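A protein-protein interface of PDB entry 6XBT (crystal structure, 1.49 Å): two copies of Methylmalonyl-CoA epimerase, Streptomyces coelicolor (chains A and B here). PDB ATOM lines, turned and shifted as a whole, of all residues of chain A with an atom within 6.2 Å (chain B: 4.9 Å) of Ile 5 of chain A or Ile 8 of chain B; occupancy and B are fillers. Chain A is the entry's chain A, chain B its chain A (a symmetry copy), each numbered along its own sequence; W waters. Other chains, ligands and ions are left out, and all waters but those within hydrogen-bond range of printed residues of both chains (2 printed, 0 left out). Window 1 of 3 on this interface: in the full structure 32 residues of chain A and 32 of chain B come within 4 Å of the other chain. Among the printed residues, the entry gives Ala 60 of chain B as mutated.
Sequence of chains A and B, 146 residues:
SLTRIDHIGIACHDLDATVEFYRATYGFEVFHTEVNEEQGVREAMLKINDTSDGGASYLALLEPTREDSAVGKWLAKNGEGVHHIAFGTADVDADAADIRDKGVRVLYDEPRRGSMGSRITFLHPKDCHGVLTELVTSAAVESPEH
Water W1 lies within hydrogen-bond range of the side-chain hydroxyl of Ser 57 of chain A, the side-chain hydroxyl of Ser 57 of chain B and the side-chain amide nitrogen of Asn 49 of chain B. Water W2 bridges the backbone carbonyl oxygen of Thr 3 of chain A and the backbone carbonyl oxygen of Ile 48 of chain B.
The backbone carbonyl oxygen (O) of Ile 8 of chain B is in hydrogen-bond range of the backbone NH (N) of Ala 60 of chain B. The backbone carbonyl oxygen of Asp 6 of chain B is in hydrogen-bond range of the backbone NH of Tyr 58 of chain B (2.9 Å). The backbone NH (N) of Ile 8 of chain A lies within hydrogen-bond range of the backbone carbonyl oxygen (O) of Tyr 58 of chain A (3.1 Å). OG1 of Thr 51 of chain A is in hydrogen-bond range of N of Ala 56 of chain A (3.3 Å). The backbone carbonyl oxygen of Asn 49 of chain B lies within hydrogen-bond range of the backbone NH of Ser 57 of chain B, at 2.9 Å. The guanidinium group of Arg 4 of chain A is in salt-bridge range of the side-chain carboxylate of Asp 6 of chain A (3.0 Å).
O of Thr 3 of chain A touches CB of Asn 49 of chain B, at 3.5 Å. Asn 49 of chain B touches Arg 4 of chain A. Ile 5 of chain A touches Ile 8 of chain B. Ile 5 of chain A touches Ile 48 of chain B (N to CG2, 3.7 Å). Ile 5 of chain A touches Tyr 58 of chain B. Ile 8 of chain A touches Ile 85 of chain B. Asn 49 of chain B touches Thr 51 of chain A. Ile 85 of chain A touches Ile 8 of chain B (CG2 to CD1, 3.9 Å). CG2 of Ile 85 of chain A touches CG2 of Val 82 of chain B, 3.9 Å away. Phe 87 of chain A touches Leu 59 of chain B.
Of the 14 printed residues of chain B, 7 touch a printed residue of chain A. Hydrophobic or aromatic side chains of chain B within 4 Å of the printed part of chain A: Ile 8, Ile 48, Leu 59, Val 82 and Ile 85. Among the printed residues, 13 pairs touch across the chains.
Of the printed residues of chain B, Ile 5 of chain A touches Ile 8 (3.9 Å), Ile 48 (3.7 Å), Asn 49 (3.0 Å) and Tyr 58 (3.8 Å). Of chain A, only Ile 5 (3.9 Å) and Ile 85 (3.9 Å) come within 4 Å of Ile 8 of chain B. Printed residues of chain B within 4 Å of Ile 85 of chain A: Ile 8 (3.9 Å) and Val 82 (3.9 Å). Printed residues of chain A within 4 Å of Asn 49 of chain B: Thr 3 (3.5 Å), Arg 4 (3.2 Å), Ile 5 (3.0 Å) and Thr 51 (3.4 Å). Of the printed residues of chain A, Tyr 58 of chain B touches Ile 5 (3.8 Å). The nearest printed residue of chain B that does not touch Ile 5 of chain A is Ser 57 of chain B (4.1 Å). The nearest residue of chain A that does not touch Ile 8 of chain B is Ile 8 of chain A (4.2 Å). The nearest printed residue of chain A that does not touch Tyr 58 of chain B is Phe 87 of chain A (7.2 Å).
The backbone carbonyl oxygen of Thr 3 of chain A sits close to the backbone carbonyl oxygen of Ile 48 of chain B (3.3 Å). The backbone NH of Ile 5 of chain A sits at hydrogen-bond distance from the side-chain amide oxygen of Asn 49 of chain B (3.0 Å).
Ile 8 of chain A touches Ile 85 of chain B, and with the chains exchanged Ile 85 of chain A touches Ile 8 of chain B. Of the 13 pairs that touch across the chains among the printed residues, 2 have their exchanged pair printed and touching as well.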
ATOM      1  N   THR A   3     -14.174 -11.979  -2.577  1.00  0.00           N
ATOM      2  CA  THR A   3     -13.577 -13.340  -2.493  1.00  0.00           C
ATOM      3  C   THR A   3     -12.920 -13.649  -1.143  1.00  0.00           C
ATOM      4  O   THR A   3     -12.480 -14.793  -0.970  1.00  0.00           O
ATOM      5  CB  THR A   3     -12.526 -13.444  -3.604  1.00  0.00           C
ATOM      6  OG1 THR A   3     -11.582 -12.416  -3.549  1.00  0.00           O
ATOM      7  CG2 THR A   3     -13.228 -13.465  -4.948  1.00  0.00           C
ATOM      8  N   ARG A   4     -12.939 -12.718  -0.156  1.00  0.00           N
ATOM      9  CA  ARG A   4     -12.432 -13.089   1.179  1.00  0.00           C
ATOM     10  C   ARG A   4     -13.013 -12.131   2.201  1.00  0.00           C
ATOM     11  O   ARG A   4     -13.448 -11.009   1.829  1.00  0.00           O
ATOM     12  CB  ARG A   4     -10.915 -12.948   1.256  1.00  0.00           C
ATOM     13  CG  ARG A   4     -10.363 -11.558   1.056  1.00  0.00           C
ATOM     14  CD  ARG A   4      -8.825 -11.458   1.126  1.00  0.00           C
ATOM     15  NE  ARG A   4      -8.340 -10.134   0.900  1.00  0.00           N
ATOM     16  CZ  ARG A   4      -8.217  -9.584  -0.311  1.00  0.00           C
ATOM     17  NH1 ARG A   4      -8.435 -10.308  -1.361  1.00  0.00           N
ATOM     18  NH2 ARG A   4      -7.843  -8.325  -0.414  1.00  0.00           N
ATOM     19  N   ILE A   5     -12.948 -12.528   3.472  1.00  0.00           N
ATOM     20  CA  ILE A   5     -12.947 -11.575   4.596  1.00  0.00           C
ATOM     21  C   ILE A   5     -11.559 -10.952   4.603  1.00  0.00           C
ATOM     22  O   ILE A   5     -10.565 -11.680   4.909  1.00  0.00           O
ATOM     23  CB  ILE A   5     -13.352 -12.252   5.900  1.00  0.00           C
ATOM     24  CG1 ILE A   5     -14.750 -12.838   5.791  1.00  0.00           C
ATOM     25  CG2 ILE A   5     -13.172 -11.266   7.047  1.00  0.00           C
ATOM     26  CD1 ILE A   5     -15.303 -13.546   7.021  1.00  0.00           C
ATOM     27  N   ASP A   6     -11.429  -9.659   4.372  1.00  0.00           N
ATOM     28  CA  ASP A   6     -10.129  -8.995   4.386  1.00  0.00           C
ATOM     29  C   ASP A   6      -9.759  -8.616   5.819  1.00  0.00           C
ATOM     30  O   ASP A   6      -8.608  -8.864   6.266  1.00  0.00           O
ATOM     31  CB  ASP A   6     -10.094  -7.760   3.488  1.00  0.00           C
ATOM     32  CG  ASP A   6      -8.699  -7.162   3.427  1.00  0.00           C
ATOM     33  OD1 ASP A   6      -7.942  -7.669   2.539  1.00  0.00           O
ATOM     34  OD2 ASP A   6      -8.445  -6.190   4.143  1.00  0.00           O
ATOM     35  N   HIS A   7     -10.643  -7.992   6.596  1.00  0.00           N
ATOM     36  CA  HIS A   7     -10.278  -7.668   7.973  1.00  0.00           C
ATOM     37  C   HIS A   7     -11.534  -7.400   8.803  1.00  0.00           C
ATOM     38  O   HIS A   7     -12.631  -7.160   8.248  1.00  0.00           O
ATOM     39  CB  HIS A   7      -9.310  -6.495   8.044  1.00  0.00           C
ATOM     40  CG  HIS A   7      -9.790  -5.167   7.534  1.00  0.00           C
ATOM     41  ND1 HIS A   7      -9.568  -4.778   6.203  1.00  0.00           N
ATOM     42  CD2 HIS A   7     -10.327  -4.107   8.176  1.00  0.00           C
ATOM     43  CE1 HIS A   7      -9.985  -3.501   6.099  1.00  0.00           C
ATOM     44  NE2 HIS A   7     -10.493  -3.067   7.247  1.00  0.00           N
ATOM     45  N   ILE A   8     -11.324  -7.358  10.087  1.00  0.00           N
ATOM     46  CA  ILE A   8     -12.313  -6.920  11.091  1.00  0.00           C
ATOM     47  C   ILE A   8     -11.749  -5.628  11.684  1.00  0.00           C
ATOM     48  O   ILE A   8     -10.591  -5.645  12.194  1.00  0.00           O
ATOM     49  CB  ILE A   8     -12.515  -7.957  12.195  1.00  0.00           C
ATOM     50  CG1 ILE A   8     -12.925  -9.320  11.604  1.00  0.00           C
ATOM     51  CG2 ILE A   8     -13.545  -7.427  13.210  1.00  0.00           C
ATOM     52  CD1 ILE A   8     -12.943 -10.476  12.550  1.00  0.00           C
ATOM     53  N   THR A  51      -5.513 -16.428   2.758  1.00  0.00           N
ATOM     54  CA  THR A  51      -6.797 -16.842   2.196  1.00  0.00           C
ATOM     55  C   THR A  51      -6.651 -17.462   0.780  1.00  0.00           C
ATOM     56  O   THR A  51      -5.668 -17.116   0.082  1.00  0.00           O
ATOM     57  CB  THR A  51      -7.749 -15.619   2.192  1.00  0.00           C
ATOM     58  OG1 THR A  51      -7.252 -14.523   1.454  1.00  0.00           O
ATOM     59  CG2 THR A  51      -8.016 -15.124   3.588  1.00  0.00           C
ATOM     60  N   ALA A  56      -5.191 -12.150   2.380  1.00  0.00           N
ATOM     61  CA  ALA A  56      -4.969 -12.441   3.815  1.00  0.00           C
ATOM     62  C   ALA A  56      -6.119 -11.857   4.609  1.00  0.00           C
ATOM     63  O   ALA A  56      -6.870 -11.000   4.064  1.00  0.00           O
ATOM     64  CB  ALA A  56      -3.666 -11.863   4.270  1.00  0.00           C
ATOM     65  N   SER A  57      -6.261 -12.305   5.860  1.00  0.00           N
ATOM     66  CA  SER A  57      -7.276 -11.801   6.809  1.00  0.00           C
ATOM     67  C   SER A  57      -6.556 -11.212   7.998  1.00  0.00           C
ATOM     68  O   SER A  57      -5.661 -11.852   8.554  1.00  0.00           O
ATOM     69  CB  SER A  57      -8.220 -12.875   7.245  1.00  0.00           C
ATOM     70  OG  SER A  57      -9.049 -13.340   6.182  1.00  0.00           O
ATOM     71  N   TYR A  58      -6.938 -10.015   8.379  1.00  0.00           N
ATOM     72  CA  TYR A  58      -6.313  -9.269   9.456  1.00  0.00           C
ATOM     73  C   TYR A  58      -7.350  -8.829  10.524  1.00  0.00           C
ATOM     74  O   TYR A  58      -8.556  -8.689  10.214  1.00  0.00           O
ATOM     75  CB  TYR A  58      -5.679  -7.969   8.908  1.00  0.00           C
ATOM     76  CG  TYR A  58      -4.698  -8.130   7.758  1.00  0.00           C
ATOM     77  CD1 TYR A  58      -3.333  -8.284   7.974  1.00  0.00           C
ATOM     78  CD2 TYR A  58      -5.165  -8.086   6.471  1.00  0.00           C
ATOM     79  CE1 TYR A  58      -2.467  -8.444   6.893  1.00  0.00           C
ATOM     80  CE2 TYR A  58      -4.301  -8.210   5.395  1.00  0.00           C
ATOM     81  CZ  TYR A  58      -2.960  -8.419   5.637  1.00  0.00           C
ATOM     82  OH  TYR A  58      -2.091  -8.506   4.563  1.00  0.00           O
ATOM     83  N   ILE A  85     -16.627  -4.475   9.247  1.00  0.00           N
ATOM     84  CA  ILE A  85     -16.087  -5.692   8.597  1.00  0.00           C
ATOM     85  C   ILE A  85     -15.691  -5.328   7.184  1.00  0.00           C
ATOM     86  O   ILE A  85     -16.301  -4.436   6.544  1.00  0.00           O
ATOM     87  CB  ILE A  85     -17.041  -6.837   8.654  1.00  0.00           C
ATOM     88  CG1 ILE A  85     -18.166  -6.682   7.689  1.00  0.00           C
ATOM     89  CG2 ILE A  85     -17.528  -7.094  10.074  1.00  0.00           C
ATOM     90  CD1 ILE A  85     -19.050  -7.946   7.719  1.00  0.00           C
ATOM     91  N   ALA A  86     -14.672  -5.945   6.635  1.00  0.00           N
ATOM     92  CA  ALA A  86     -14.193  -5.647   5.298  1.00  0.00           C
ATOM     93  C   ALA A  86     -14.053  -6.898   4.455  1.00  0.00           C
ATOM     94  O   ALA A  86     -13.498  -7.892   4.927  1.00  0.00           O
ATOM     95  CB  ALA A  86     -12.854  -4.947   5.345  1.00  0.00           C
ATOM     96  N   PHE A  87     -14.494  -6.826   3.226  1.00  0.00           N
ATOM     97  CA  PHE A  87     -14.404  -7.893   2.233  1.00  0.00           C
ATOM     98  C   PHE A  87     -13.383  -7.485   1.179  1.00  0.00           C
ATOM     99  O   PHE A  87     -13.357  -6.353   0.723  1.00  0.00           O
ATOM    100  CB  PHE A  87     -15.748  -8.157   1.592  1.00  0.00           C
ATOM    101  CG  PHE A  87     -16.771  -8.671   2.557  1.00  0.00           C
ATOM    102  CD1 PHE A  87     -16.719  -9.914   3.110  1.00  0.00           C
ATOM    103  CD2 PHE A  87     -17.845  -7.870   2.880  1.00  0.00           C
ATOM    104  CE1 PHE A  87     -17.670 -10.333   4.012  1.00  0.00           C
ATOM    105  CE2 PHE A  87     -18.811  -8.285   3.791  1.00  0.00           C
ATOM    106  CZ  PHE A  87     -18.691  -9.514   4.380  1.00  0.00           C
ATOM    107  N   GLY A  88     -12.581  -8.444   0.758  1.00  0.00           N
ATOM    108  CA  GLY A  88     -11.589  -8.202  -0.315  1.00  0.00           C
ATOM    109  C   GLY A  88     -12.135  -8.578  -1.676  1.00  0.00           C
ATOM    110  O   GLY A  88     -12.964  -9.483  -1.795  1.00  0.00           O
ATOM    111  N   ASP B   6     -12.305 -17.701  12.049  1.00  0.00           N
ATOM    112  CA  ASP B   6     -13.261 -18.740  11.680  1.00  0.00           C
ATOM    113  C   ASP B   6     -14.566 -18.098  11.210  1.00  0.00           C
ATOM    114  O   ASP B   6     -15.126 -18.496  10.154  1.00  0.00           O
ATOM    115  CB  ASP B   6     -13.536 -19.714  12.824  1.00  0.00           C
ATOM    116  CG  ASP B   6     -14.437 -20.852  12.377  1.00  0.00           C
ATOM    117  OD1 ASP B   6     -13.826 -21.839  11.856  1.00  0.00           O
ATOM    118  OD2 ASP B   6     -15.640 -20.786  12.639  1.00  0.00           O
ATOM    119  N   HIS B   7     -15.135 -17.134  11.931  1.00  0.00           N
ATOM    120  CA  HIS B   7     -16.365 -16.513  11.445  1.00  0.00           C
ATOM    121  C   HIS B   7     -16.586 -15.167  12.137  1.00  0.00           C
ATOM    122  O   HIS B   7     -15.973 -14.879  13.191  1.00  0.00           O
ATOM    123  CB  HIS B   7     -17.570 -17.426  11.619  1.00  0.00           C
ATOM    124  CG  HIS B   7     -17.954 -17.810  13.019  1.00  0.00           C
ATOM    125  ND1 HIS B   7     -17.458 -18.984  13.610  1.00  0.00           N
ATOM    126  CD2 HIS B   7     -18.865 -17.288  13.869  1.00  0.00           C
ATOM    127  CE1 HIS B   7     -18.089 -19.116  14.794  1.00  0.00           C
ATOM    128  NE2 HIS B   7     -18.911 -18.097  15.016  1.00  0.00           N
ATOM    129  N   ILE B   8     -17.507 -14.431  11.587  1.00  0.00           N
ATOM    130  CA  ILE B   8     -18.056 -13.189  12.166  1.00  0.00           C
ATOM    131  C   ILE B   8     -19.516 -13.502  12.497  1.00  0.00           C
ATOM    132  O   ILE B   8     -20.274 -13.922  11.575  1.00  0.00           O
ATOM    133  CB  ILE B   8     -17.980 -12.014  11.193  1.00  0.00           C
ATOM    134  CG1 ILE B   8     -16.533 -11.784  10.715  1.00  0.00           C
ATOM    135  CG2 ILE B   8     -18.581 -10.762  11.859  1.00  0.00           C
ATOM    136  CD1 ILE B   8     -16.349 -10.809   9.599  1.00  0.00           C
ATOM    137  N   GLY B   9     -19.927 -13.393  13.744  1.00  0.00           N
ATOM    138  CA  GLY B   9     -21.303 -13.628  14.187  1.00  0.00           C
ATOM    139  C   GLY B   9     -22.094 -12.357  14.050  1.00  0.00           C
ATOM    140  O   GLY B   9     -21.674 -11.298  14.631  1.00  0.00           O
ATOM    141  N   ILE B  10     -23.121 -12.350  13.240  1.00  0.00           N
ATOM    142  CA  ILE B  10     -23.917 -11.152  12.933  1.00  0.00           C
ATOM    143  C   ILE B  10     -25.357 -11.410  13.353  1.00  0.00           C
ATOM    144  O   ILE B  10     -25.960 -12.341  12.854  1.00  0.00           O
ATOM    145  CB  ILE B  10     -23.813 -10.860  11.433  1.00  0.00           C
ATOM    146  CG1 ILE B  10     -22.355 -10.513  11.061  1.00  0.00           C
ATOM    147  CG2 ILE B  10     -24.811  -9.767  11.041  1.00  0.00           C
ATOM    148  CD1 ILE B  10     -22.095 -10.435   9.581  1.00  0.00           C
ATOM    149  N   ILE B  48     -17.151 -17.614   2.924  1.00  0.00           N
ATOM    150  CA  ILE B  48     -16.547 -16.520   2.132  1.00  0.00           C
ATOM    151  C   ILE B  48     -15.256 -16.990   1.476  1.00  0.00           C
ATOM    152  O   ILE B  48     -14.974 -16.575   0.324  1.00  0.00           O
ATOM    153  CB  ILE B  48     -16.359 -15.256   2.999  1.00  0.00           C
ATOM    154  CG1 ILE B  48     -17.620 -14.926   3.806  1.00  0.00           C
ATOM    155  CG2 ILE B  48     -15.968 -14.079   2.105  1.00  0.00           C
ATOM    156  CD1 ILE B  48     -18.897 -14.815   3.013  1.00  0.00           C
ATOM    157  N   ASN B  49     -14.443 -17.806   2.180  1.00  0.00           N
ATOM    158  CA  ASN B  49     -13.110 -18.200   1.636  1.00  0.00           C
ATOM    159  C   ASN B  49     -12.606 -19.396   2.437  1.00  0.00           C
ATOM    160  O   ASN B  49     -13.087 -19.660   3.580  1.00  0.00           O
ATOM    161  CB  ASN B  49     -12.115 -17.068   1.599  1.00  0.00           C
ATOM    162  CG  ASN B  49     -11.898 -16.469   2.979  1.00  0.00           C
ATOM    163  OD1 ASN B  49     -12.586 -15.492   3.322  1.00  0.00           O
ATOM    164  ND2 ASN B  49     -10.891 -16.929   3.699  1.00  0.00           N
ATOM    165  N   SER B  57     -13.465 -19.435   6.430  1.00  0.00           N
ATOM    166  CA  SER B  57     -14.013 -18.231   7.091  1.00  0.00           C
ATOM    167  C   SER B  57     -15.438 -18.049   6.629  1.00  0.00           C
ATOM    168  O   SER B  57     -15.706 -18.095   5.427  1.00  0.00           O
ATOM    169  CB  SER B  57     -13.203 -17.010   6.794  1.00  0.00           C
ATOM    170  OG  SER B  57     -11.899 -17.065   7.366  1.00  0.00           O
ATOM    171  N   TYR B  58     -16.335 -17.849   7.566  1.00  0.00           N
ATOM    172  CA  TYR B  58     -17.759 -17.721   7.312  1.00  0.00           C
ATOM    173  C   TYR B  58     -18.331 -16.404   7.902  1.00  0.00           C
ATOM    174  O   TYR B  58     -17.762 -15.847   8.870  1.00  0.00           O
ATOM    175  CB  TYR B  58     -18.529 -18.873   8.001  1.00  0.00           C
ATOM    176  CG  TYR B  58     -18.072 -20.283   7.668  1.00  0.00           C
ATOM    177  CD1 TYR B  58     -18.631 -21.010   6.623  1.00  0.00           C
ATOM    178  CD2 TYR B  58     -17.106 -20.872   8.442  1.00  0.00           C
ATOM    179  CE1 TYR B  58     -18.175 -22.296   6.340  1.00  0.00           C
ATOM    180  CE2 TYR B  58     -16.675 -22.164   8.183  1.00  0.00           C
ATOM    181  CZ  TYR B  58     -17.205 -22.840   7.106  1.00  0.00           C
ATOM    182  OH  TYR B  58     -16.803 -24.143   6.869  1.00  0.00           O
ATOM    183  N   LEU B  59     -19.476 -16.006   7.381  1.00  0.00           N
ATOM    184  CA  LEU B  59     -20.412 -15.114   8.101  1.00  0.00           C
ATOM    185  C   LEU B  59     -21.440 -15.999   8.762  1.00  0.00           C
ATOM    186  O   LEU B  59     -22.017 -16.872   8.051  1.00  0.00           O
ATOM    187  CB  LEU B  59     -21.071 -14.121   7.168  1.00  0.00           C
ATOM    188  CG  LEU B  59     -20.101 -13.295   6.367  1.00  0.00           C
ATOM    189  CD1 LEU B  59     -20.880 -12.417   5.416  1.00  0.00           C
ATOM    190  CD2 LEU B  59     -19.207 -12.447   7.246  1.00  0.00           C
ATOM    191  N   ALA B  60     -21.652 -15.918  10.067  1.00  0.00           N
ATOM    192  CA  ALA B  60     -22.657 -16.670  10.805  1.00  0.00           C
ATOM    193  C   ALA B  60     -23.795 -15.715  11.118  1.00  0.00           C
ATOM    194  O   ALA B  60     -23.644 -14.853  12.004  1.00  0.00           O
ATOM    195  CB  ALA B  60     -22.059 -17.255  12.018  1.00  0.00           C
ATOM    196  N   VAL B  82     -22.935  -6.649  14.211  1.00  0.00           N
ATOM    197  CA  VAL B  82     -21.953  -7.646  14.641  1.00  0.00           C
ATOM    198  C   VAL B  82     -22.115  -7.994  16.115  1.00  0.00           C
ATOM    199  O   VAL B  82     -21.995  -7.064  16.941  1.00  0.00           O
ATOM    200  CB  VAL B  82     -20.519  -7.195  14.326  1.00  0.00           C
ATOM    201  CG1 VAL B  82     -19.519  -8.242  14.799  1.00  0.00           C
ATOM    202  CG2 VAL B  82     -20.320  -6.898  12.847  1.00  0.00           C
ATOM    203  N   HIS B  84     -20.294 -11.030  17.532  1.00  0.00           N
ATOM    204  CA  HIS B  84     -19.049 -11.652  18.037  1.00  0.00           C
ATOM    205  C   HIS B  84     -18.099 -11.943  16.883  1.00  0.00           C
ATOM    206  O   HIS B  84     -18.540 -11.945  15.753  1.00  0.00           O
ATOM    207  CB  HIS B  84     -19.334 -12.911  18.870  1.00  0.00           C
ATOM    208  CG  HIS B  84     -19.887 -14.066  18.126  1.00  0.00           C
ATOM    209  ND1 HIS B  84     -21.244 -14.291  18.057  1.00  0.00           N
ATOM    210  CD2 HIS B  84     -19.283 -15.120  17.543  1.00  0.00           C
ATOM    211  CE1 HIS B  84     -21.400 -15.451  17.407  1.00  0.00           C
ATOM    212  NE2 HIS B  84     -20.245 -15.993  17.076  1.00  0.00           N
ATOM    213  N   ILE B  85     -16.866 -12.221  17.229  1.00  0.00           N
ATOM    214  CA  ILE B  85     -15.846 -12.708  16.272  1.00  0.00           C
ATOM    215  C   ILE B  85     -15.348 -14.049  16.765  1.00  0.00           C
ATOM    216  O   ILE B  85     -15.307 -14.320  17.990  1.00  0.00           O
ATOM    217  CB  ILE B  85     -14.745 -11.724  16.064  1.00  0.00           C
ATOM    218  CG1 ILE B  85     -13.805 -11.677  17.219  1.00  0.00           C
ATOM    219  CG2 ILE B  85     -15.284 -10.346  15.701  1.00  0.00           C
ATOM    220  CD1 ILE B  85     -12.634 -10.726  16.894  1.00  0.00           C
HETATM  221  O   HOH W   1      -9.982 -15.740   6.267  1.00  0.00           O
HETATM  222  O   HOH W   2     -13.169 -17.073  -2.297  1.00  0.00           O
